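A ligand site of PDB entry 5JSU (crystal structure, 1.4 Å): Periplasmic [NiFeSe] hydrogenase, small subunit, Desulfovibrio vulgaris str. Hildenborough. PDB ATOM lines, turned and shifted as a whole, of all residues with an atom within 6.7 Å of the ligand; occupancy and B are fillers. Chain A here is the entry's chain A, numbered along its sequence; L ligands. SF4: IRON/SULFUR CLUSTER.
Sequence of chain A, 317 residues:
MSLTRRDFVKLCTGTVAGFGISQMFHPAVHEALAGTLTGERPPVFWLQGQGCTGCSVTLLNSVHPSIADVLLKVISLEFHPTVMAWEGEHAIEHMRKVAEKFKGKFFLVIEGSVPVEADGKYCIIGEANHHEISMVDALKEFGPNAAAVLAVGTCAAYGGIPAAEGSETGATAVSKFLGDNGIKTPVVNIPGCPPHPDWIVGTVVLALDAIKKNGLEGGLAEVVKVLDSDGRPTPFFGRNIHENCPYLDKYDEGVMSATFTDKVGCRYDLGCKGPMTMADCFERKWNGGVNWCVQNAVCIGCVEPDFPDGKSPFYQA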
ATOM      1  N   ILE A 241     -26.482  16.119  22.523  1.00  0.00           N
ATOM      2  CA  ILE A 241     -25.133  16.143  23.084  1.00  0.00           C
ATOM      3  C   ILE A 241     -24.231  15.132  22.381  1.00  0.00           C
ATOM      4  O   ILE A 241     -23.149  15.467  21.893  1.00  0.00           O
ATOM      5  CB  ILE A 241     -25.188  15.865  24.600  1.00  0.00           C
ATOM      6  CG1 ILE A 241     -25.862  17.009  25.371  1.00  0.00           C
ATOM      7  CG2 ILE A 241     -23.798  15.577  25.158  1.00  0.00           C
ATOM      8  CD1 ILE A 241     -25.021  18.276  25.552  1.00  0.00           C
ATOM      9  N   HIS A 242     -24.675  13.874  22.329  1.00  0.00           N
ATOM     10  CA  HIS A 242     -23.843  12.769  21.861  1.00  0.00           C
ATOM     11  C   HIS A 242     -23.471  12.884  20.386  1.00  0.00           C
ATOM     12  O   HIS A 242     -22.311  12.665  20.010  1.00  0.00           O
ATOM     13  CB  HIS A 242     -24.638  11.500  22.149  1.00  0.00           C
ATOM     14  CG  HIS A 242     -24.046  10.233  21.598  1.00  0.00           C
ATOM     15  ND1 HIS A 242     -22.997   9.560  22.209  1.00  0.00           N
ATOM     16  CD2 HIS A 242     -24.393   9.507  20.514  1.00  0.00           C
ATOM     17  CE1 HIS A 242     -22.738   8.468  21.516  1.00  0.00           C
ATOM     18  NE2 HIS A 242     -23.562   8.415  20.481  1.00  0.00           N
ATOM     19  N   GLU A 243     -24.432  13.242  19.541  1.00  0.00           N
ATOM     20  CA  GLU A 243     -24.146  13.294  18.113  1.00  0.00           C
ATOM     21  C   GLU A 243     -23.183  14.428  17.779  1.00  0.00           C
ATOM     22  O   GLU A 243     -22.605  14.435  16.690  1.00  0.00           O
ATOM     23  CB  GLU A 243     -25.429  13.430  17.291  1.00  0.00           C
ATOM     24  CG  GLU A 243     -26.376  12.238  17.427  1.00  0.00           C
ATOM     25  CD  GLU A 243     -25.778  10.921  16.964  1.00  0.00           C
ATOM     26  OE1 GLU A 243     -26.198   9.875  17.486  1.00  0.00           O
ATOM     27  OE2 GLU A 243     -24.896  10.917  16.080  1.00  0.00           O
ATOM     28  N   CYS A 245     -20.648  15.214  20.089  1.00  0.00           N
ATOM     29  CA  CYS A 245     -19.648  15.076  21.124  1.00  0.00           C
ATOM     30  C   CYS A 245     -18.262  14.814  20.542  1.00  0.00           C
ATOM     31  O   CYS A 245     -18.115  14.012  19.599  1.00  0.00           O
ATOM     32  CB  CYS A 245     -19.995  13.929  22.049  1.00  0.00           C
ATOM     33  SG  CYS A 245     -18.799  13.677  23.402  1.00  0.00           S
ATOM     34  N   PRO A 246     -17.218  15.443  21.082  1.00  0.00           N
ATOM     35  CA  PRO A 246     -15.869  15.178  20.555  1.00  0.00           C
ATOM     36  C   PRO A 246     -15.357  13.778  20.814  1.00  0.00           C
ATOM     37  O   PRO A 246     -14.347  13.403  20.217  1.00  0.00           O
ATOM     38  CB  PRO A 246     -14.998  16.226  21.258  1.00  0.00           C
ATOM     39  CG  PRO A 246     -15.710  16.559  22.465  1.00  0.00           C
ATOM     40  CD  PRO A 246     -17.197  16.457  22.142  1.00  0.00           C
ATOM     41  N   TYR A 247     -16.016  12.975  21.665  1.00  0.00           N
ATOM     42  CA  TYR A 247     -15.595  11.601  21.927  1.00  0.00           C
ATOM     43  C   TYR A 247     -16.423  10.594  21.157  1.00  0.00           C
ATOM     44  O   TYR A 247     -16.278   9.387  21.379  1.00  0.00           O
ATOM     45  CB  TYR A 247     -15.586  11.319  23.446  1.00  0.00           C
ATOM     46  CG  TYR A 247     -14.878  12.425  24.192  1.00  0.00           C
ATOM     47  CD1 TYR A 247     -13.529  12.661  24.019  1.00  0.00           C
ATOM     48  CD2 TYR A 247     -15.596  13.285  25.019  1.00  0.00           C
ATOM     49  CE1 TYR A 247     -12.910  13.712  24.674  1.00  0.00           C
ATOM     50  CE2 TYR A 247     -14.983  14.331  25.662  1.00  0.00           C
ATOM     51  CZ  TYR A 247     -13.642  14.546  25.494  1.00  0.00           C
ATOM     52  OH  TYR A 247     -13.053  15.610  26.133  1.00  0.00           O
ATOM     53  N   LEU A 248     -17.242  11.067  20.219  1.00  0.00           N
ATOM     54  CA  LEU A 248     -18.106  10.171  19.462  1.00  0.00           C
ATOM     55  C   LEU A 248     -17.323   9.130  18.682  1.00  0.00           C
ATOM     56  O   LEU A 248     -17.777   7.980  18.552  1.00  0.00           O
ATOM     57  CB  LEU A 248     -19.013  10.994  18.552  1.00  0.00           C
ATOM     58  CG  LEU A 248     -20.076  10.250  17.757  1.00  0.00           C
ATOM     59  CD1 LEU A 248     -21.041   9.495  18.681  1.00  0.00           C
ATOM     60  CD2 LEU A 248     -20.818  11.232  16.859  1.00  0.00           C
ATOM     61  N   ASP A 249     -16.151   9.472  18.167  1.00  0.00           N
ATOM     62  CA  ASP A 249     -15.353   8.471  17.456  1.00  0.00           C
ATOM     63  C   ASP A 249     -14.942   7.337  18.392  1.00  0.00           C
ATOM     64  O   ASP A 249     -14.919   6.166  17.981  1.00  0.00           O
ATOM     65  CB  ASP A 249     -14.170   9.119  16.730  1.00  0.00           C
ATOM     66  CG  ASP A 249     -13.216   9.869  17.643  1.00  0.00           C
ATOM     67  OD1 ASP A 249     -13.593  10.284  18.771  1.00  0.00           O
ATOM     68  OD2 ASP A 249     -12.048  10.069  17.203  1.00  0.00           O
ATOM     69  N   LYS A 250     -14.637   7.653  19.648  1.00  0.00           N
ATOM     70  CA  LYS A 250     -14.275   6.621  20.606  1.00  0.00           C
ATOM     71  C   LYS A 250     -15.475   5.755  20.956  1.00  0.00           C
ATOM     72  O   LYS A 250     -15.348   4.522  21.036  1.00  0.00           O
ATOM     73  CB  LYS A 250     -13.688   7.250  21.882  1.00  0.00           C
ATOM     74  CG  LYS A 250     -12.447   8.074  21.607  1.00  0.00           C
ATOM     75  CD  LYS A 250     -11.330   7.218  21.082  1.00  0.00           C
ATOM     76  CE  LYS A 250     -10.095   8.030  20.833  1.00  0.00           C
ATOM     77  NZ  LYS A 250      -8.971   7.128  20.462  1.00  0.00           N
ATOM     78  N   TYR A 251     -16.645   6.361  21.139  1.00  0.00           N
ATOM     79  CA  TYR A 251     -17.872   5.591  21.331  1.00  0.00           C
ATOM     80  C   TYR A 251     -18.056   4.581  20.209  1.00  0.00           C
ATOM     81  O   TYR A 251     -18.265   3.391  20.466  1.00  0.00           O
ATOM     82  CB  TYR A 251     -19.063   6.543  21.386  1.00  0.00           C
ATOM     83  CG  TYR A 251     -20.395   5.827  21.463  1.00  0.00           C
ATOM     84  CD1 TYR A 251     -20.956   5.485  22.685  1.00  0.00           C
ATOM     85  CD2 TYR A 251     -21.123   5.517  20.310  1.00  0.00           C
ATOM     86  CE1 TYR A 251     -22.176   4.843  22.763  1.00  0.00           C
ATOM     87  CE2 TYR A 251     -22.330   4.874  20.383  1.00  0.00           C
ATOM     88  CZ  TYR A 251     -22.863   4.538  21.612  1.00  0.00           C
ATOM     89  OH  TYR A 251     -24.076   3.901  21.703  1.00  0.00           O
ATOM     90  N   ASP A 252     -17.967   5.037  18.965  1.00  0.00           N
ATOM     91  CA  ASP A 252     -18.189   4.135  17.823  1.00  0.00           C
ATOM     92  C   ASP A 252     -17.115   3.057  17.749  1.00  0.00           C
ATOM     93  O   ASP A 252     -17.390   1.951  17.262  1.00  0.00           O
ATOM     94  CB  ASP A 252     -18.262   4.918  16.511  1.00  0.00           C
ATOM     95  CG  ASP A 252     -19.563   5.692  16.334  1.00  0.00           C
ATOM     96  OD1 ASP A 252     -20.586   5.342  16.961  1.00  0.00           O
ATOM     97  OD2 ASP A 252     -19.552   6.665  15.556  1.00  0.00           O
ATOM     98  N   MET A 256     -13.664   2.867  25.698  1.00  0.00           N
ATOM     99  CA  MET A 256     -14.395   3.388  26.839  1.00  0.00           C
ATOM    100  C   MET A 256     -13.429   3.566  27.993  1.00  0.00           C
ATOM    101  O   MET A 256     -12.694   2.648  28.356  1.00  0.00           O
ATOM    102  CB  MET A 256     -15.469   2.388  27.286  1.00  0.00           C
ATOM    103  CG  MET A 256     -16.503   2.119  26.243  1.00  0.00           C
ATOM    104  SD  MET A 256     -17.470   3.607  25.999  1.00  0.00           S
ATOM    105  CE  MET A 256     -18.451   3.109  24.565  1.00  0.00           C
ATOM    106  N   GLY A 265     -10.910   8.131  26.330  1.00  0.00           N
ATOM    107  CA  GLY A 265     -12.022   7.299  25.944  1.00  0.00           C
ATOM    108  C   GLY A 265     -13.359   7.968  26.076  1.00  0.00           C
ATOM    109  O   GLY A 265     -13.508   9.045  26.656  1.00  0.00           O
ATOM    110  N   CYS A 266     -14.365   7.299  25.509  1.00  0.00           N
ATOM    111  CA  CYS A 266     -15.745   7.710  25.710  1.00  0.00           C
ATOM    112  C   CYS A 266     -16.173   7.393  27.151  1.00  0.00           C
ATOM    113  O   CYS A 266     -15.659   6.456  27.780  1.00  0.00           O
ATOM    114  CB  CYS A 266     -16.630   7.011  24.669  1.00  0.00           C
ATOM    115  SG  CYS A 266     -18.424   7.009  24.975  1.00  0.00           S
ATOM    116  N   ARG A 267     -17.097   8.205  27.662  1.00  0.00           N
ATOM    117  CA  ARG A 267     -17.567   8.139  29.038  1.00  0.00           C
ATOM    118  C   ARG A 267     -18.840   7.296  29.218  1.00  0.00           C
ATOM    119  O   ARG A 267     -19.416   7.261  30.319  1.00  0.00           O
ATOM    120  CB  ARG A 267     -17.837   9.547  29.552  1.00  0.00           C
ATOM    121  CG  ARG A 267     -16.601  10.414  29.812  1.00  0.00           C
ATOM    122  CD  ARG A 267     -15.813  10.847  28.583  1.00  0.00           C
ATOM    123  NE  ARG A 267     -15.044  12.048  28.910  1.00  0.00           N
ATOM    124  CZ  ARG A 267     -13.872  12.400  28.392  1.00  0.00           C
ATOM    125  NH1 ARG A 267     -13.256  11.638  27.480  1.00  0.00           N
ATOM    126  NH2 ARG A 267     -13.325  13.529  28.799  1.00  0.00           N
ATOM    127  N   TYR A 268     -19.291   6.617  28.169  1.00  0.00           N
ATOM    128  CA  TYR A 268     -20.548   5.868  28.229  1.00  0.00           C
ATOM    129  C   TYR A 268     -20.562   4.830  29.357  1.00  0.00           C
ATOM    130  O   TYR A 268     -21.549   4.715  30.102  1.00  0.00           O
ATOM    131  CB  TYR A 268     -20.772   5.202  26.896  1.00  0.00           C
ATOM    132  CG  TYR A 268     -22.056   4.445  26.837  1.00  0.00           C
ATOM    133  CD1 TYR A 268     -23.256   5.092  26.620  1.00  0.00           C
ATOM    134  CD2 TYR A 268     -22.087   3.065  27.015  1.00  0.00           C
ATOM    135  CE1 TYR A 268     -24.431   4.413  26.571  1.00  0.00           C
ATOM    136  CE2 TYR A 268     -23.258   2.364  26.965  1.00  0.00           C
ATOM    137  CZ  TYR A 268     -24.435   3.048  26.754  1.00  0.00           C
ATOM    138  OH  TYR A 268     -25.610   2.360  26.709  1.00  0.00           O
ATOM    139  N   ASP A 269     -19.492   4.045  29.499  1.00  0.00           N
ATOM    140  CA  ASP A 269     -19.486   3.021  30.550  1.00  0.00           C
ATOM    141  C   ASP A 269     -19.492   3.628  31.946  1.00  0.00           C
ATOM    142  O   ASP A 269     -19.934   2.981  32.896  1.00  0.00           O
ATOM    143  CB  ASP A 269     -18.289   2.093  30.420  1.00  0.00           C
ATOM    144  CG  ASP A 269     -18.417   1.092  29.282  1.00  0.00           C
ATOM    145  OD1 ASP A 269     -19.502   1.001  28.662  1.00  0.00           O
ATOM    146  OD2 ASP A 269     -17.425   0.378  29.053  1.00  0.00           O
ATOM    147  N   CYS A 272     -22.323   8.184  31.160  1.00  0.00           N
ATOM    148  CA  CYS A 272     -22.700   9.371  30.398  1.00  0.00           C
ATOM    149  C   CYS A 272     -24.075   9.205  29.734  1.00  0.00           C
ATOM    150  O   CYS A 272     -24.324   8.204  29.048  1.00  0.00           O
ATOM    151  CB  CYS A 272     -21.637   9.669  29.342  1.00  0.00           C
ATOM    152  SG  CYS A 272     -21.929  11.205  28.412  1.00  0.00           S
ATOM    153  N   LYS A 273     -24.938  10.208  29.902  1.00  0.00           N
ATOM    154  CA  LYS A 273     -26.295  10.210  29.351  1.00  0.00           C
ATOM    155  C   LYS A 273     -26.416  11.110  28.124  1.00  0.00           C
ATOM    156  O   LYS A 273     -27.530  11.427  27.690  1.00  0.00           O
ATOM    157  CB  LYS A 273     -27.309  10.604  30.425  1.00  0.00           C
ATOM    158  CG  LYS A 273     -27.310   9.682  31.650  1.00  0.00           C
ATOM    159  CD  LYS A 273     -27.423   8.218  31.289  1.00  0.00           C
ATOM    160  CE  LYS A 273     -27.623   7.335  32.517  1.00  0.00           C
ATOM    161  NZ  LYS A 273     -26.609   7.566  33.578  1.00  0.00           N
ATOM    162  N   GLY A 274     -25.276  11.536  27.555  1.00  0.00           N
ATOM    163  CA  GLY A 274     -25.306  12.321  26.348  1.00  0.00           C
ATOM    164  C   GLY A 274     -26.198  11.794  25.251  1.00  0.00           C
ATOM    165  O   GLY A 274     -26.857  12.588  24.567  1.00  0.00           O
ATOM    166  N   PRO A 275     -26.240  10.483  25.016  1.00  0.00           N
ATOM    167  CA  PRO A 275     -27.106   9.964  23.936  1.00  0.00           C
ATOM    168  C   PRO A 275     -28.563  10.358  24.082  1.00  0.00           C
ATOM    169  O   PRO A 275     -29.256  10.483  23.060  1.00  0.00           O
ATOM    170  CB  PRO A 275     -26.914   8.456  24.018  1.00  0.00           C
ATOM    171  CG  PRO A 275     -25.535   8.275  24.576  1.00  0.00           C
ATOM    172  CD  PRO A 275     -25.348   9.423  25.557  1.00  0.00           C
ATOM    173  N   TRP A 292     -16.850  21.501  30.769  1.00  0.00           N
ATOM    174  CA  TRP A 292     -18.232  21.045  30.697  1.00  0.00           C
ATOM    175  C   TRP A 292     -18.288  19.615  31.212  1.00  0.00           C
ATOM    176  O   TRP A 292     -17.272  18.978  31.437  1.00  0.00           O
ATOM    177  CB  TRP A 292     -18.835  21.154  29.297  1.00  0.00           C
ATOM    178  CG  TRP A 292     -18.288  20.262  28.239  1.00  0.00           C
ATOM    179  CD1 TRP A 292     -16.993  20.210  27.794  1.00  0.00           C
ATOM    180  CD2 TRP A 292     -19.029  19.330  27.450  1.00  0.00           C
ATOM    181  NE1 TRP A 292     -16.893  19.284  26.767  1.00  0.00           N
ATOM    182  CE2 TRP A 292     -18.127  18.741  26.532  1.00  0.00           C
ATOM    183  CE3 TRP A 292     -20.372  18.945  27.411  1.00  0.00           C
ATOM    184  CZ2 TRP A 292     -18.514  17.781  25.601  1.00  0.00           C
ATOM    185  CZ3 TRP A 292     -20.760  17.993  26.475  1.00  0.00           C
ATOM    186  CH2 TRP A 292     -19.836  17.426  25.580  1.00  0.00           C
ATOM    187  N   VAL A 294     -19.126  16.586  30.259  1.00  0.00           N
ATOM    188  CA  VAL A 294     -18.580  15.399  29.594  1.00  0.00           C
ATOM    189  C   VAL A 294     -17.056  15.392  29.643  1.00  0.00           C
ATOM    190  O   VAL A 294     -16.448  14.343  29.840  1.00  0.00           O
ATOM    191  CB  VAL A 294     -19.119  15.285  28.166  1.00  0.00           C
ATOM    192  CG1 VAL A 294     -18.444  14.126  27.435  1.00  0.00           C
ATOM    193  CG2 VAL A 294     -20.605  15.086  28.162  1.00  0.00           C
ATOM    194  N   ALA A 297     -16.356  14.795  33.642  1.00  0.00           N
ATOM    195  CA  ALA A 297     -16.885  13.582  34.253  1.00  0.00           C
ATOM    196  C   ALA A 297     -17.863  12.936  33.282  1.00  0.00           C
ATOM    197  O   ALA A 297     -17.429  12.345  32.296  1.00  0.00           O
ATOM    198  CB  ALA A 297     -17.511  13.906  35.608  1.00  0.00           C
ATOM    199  N   VAL A 298     -19.182  13.045  33.551  1.00  0.00           N
ATOM    200  CA  VAL A 298     -20.221  12.517  32.671  1.00  0.00           C
ATOM    201  C   VAL A 298     -21.342  13.544  32.578  1.00  0.00           C
ATOM    202  O   VAL A 298     -21.505  14.383  33.479  1.00  0.00           O
ATOM    203  CB  VAL A 298     -20.803  11.174  33.188  1.00  0.00           C
ATOM    204  CG1 VAL A 298     -19.722  10.076  33.248  1.00  0.00           C
ATOM    205  CG2 VAL A 298     -21.455  11.340  34.559  1.00  0.00           C
ATOM    206  N   CYS A 299     -22.130  13.468  31.507  1.00  0.00           N
ATOM    207  CA  CYS A 299     -23.423  14.131  31.454  1.00  0.00           C
ATOM    208  C   CYS A 299     -24.433  13.298  32.222  1.00  0.00           C
ATOM    209  O   CYS A 299     -24.460  12.067  32.099  1.00  0.00           O
ATOM    210  CB  CYS A 299     -23.860  14.294  29.993  1.00  0.00           C
ATOM    211  SG  CYS A 299     -25.537  14.983  29.712  1.00  0.00           S
HETATM  212 FE1  SF4 L   1     -21.057  10.688  26.340  1.00  0.00          FE
HETATM  213 FE2  SF4 L   1     -21.693  10.049  23.741  1.00  0.00          FE
HETATM  214 FE3  SF4 L   1     -19.419   9.052  24.773  1.00  0.00          FE
HETATM  215 FE4  SF4 L   1     -19.682  11.735  24.237  1.00  0.00          FE
HETATM  216  S1  SF4 L   1     -19.623  10.014  22.726  1.00  0.00           S
HETATM  217  S2  SF4 L   1     -18.753  10.776  26.118  1.00  0.00           S
HETATM  218  S3  SF4 L   1     -21.908  12.098  24.757  1.00  0.00           S
HETATM  219  S4  SF4 L   1     -21.559   8.604  25.516  1.00  0.00           S
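The backbone carbonyl oxygen of Tyr 247 lies close to a sulfur (S1) of the ligand, 3.7 Å away. Ile 241 touches the ligand. Tyr 251 touches the ligand. CB of Tyr 268 touches S4 of the ligand (3.8 Å). Gly 274 touches the ligand. Pro 275 touches the ligand (CD to S4, 3.9 Å). Val 294 touches the ligand (CG1 to S2, 3.6 Å). Hydrophobic or aromatic side chains within 4 Å of the ligand: Ile 241, His 242, Tyr 251, Tyr 268, Pro 275 and Val 294. The nearest printed residue that does not touch the ligand is Lys 273 (5.3 Å).
An iron atom (FE2) of the ligand is bound by a ring nitrogen (ND1) of His 242. An iron atom (FE3) of the ligand is bound by the side-chain sulfur (SG) of Cys 266 (2.3 Å). An iron atom (FE4) of the ligand is bound by the side-chain sulfur of Cys 245, at 2.3 Å. FE1 of the ligand is bound by SG of Cys 272, at 2.3 Å. The backbone NH (N) of Arg 267 lies close to a sulfur (S2) of the ligand (3.4 Å). The backbone NH of Leu 248 sits close to a sulfur (S1) of the ligand (3.6 Å).
The side-chain sulfur (SG) of Cys 266 sits close to the backbone NH (N) of Tyr 268, 3.3 Å away. SD of Met 256 lies close to SG of Cys 266, at 3.7 Å. The backbone NH of Tyr 247 lies close to the side-chain sulfur of Cys 245 (3.4 Å). N of Cys 272 sits at hydrogen-bond distance from O of Arg 267. SG of Cys 272 lies close to N of Gly 274 (3.5 Å). NH2 of Arg 267 sits at hydrogen-bond distance from OH of Tyr 247 (3.4 Å). The backbone carbonyl oxygen (O) of Val 294 sits at hydrogen-bond distance from the guanidinium group (NE) of Arg 267, 2.8 Å away. NH1 of Arg 267 lies within hydrogen-bond range of O of Gly 265 (2.7 Å).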
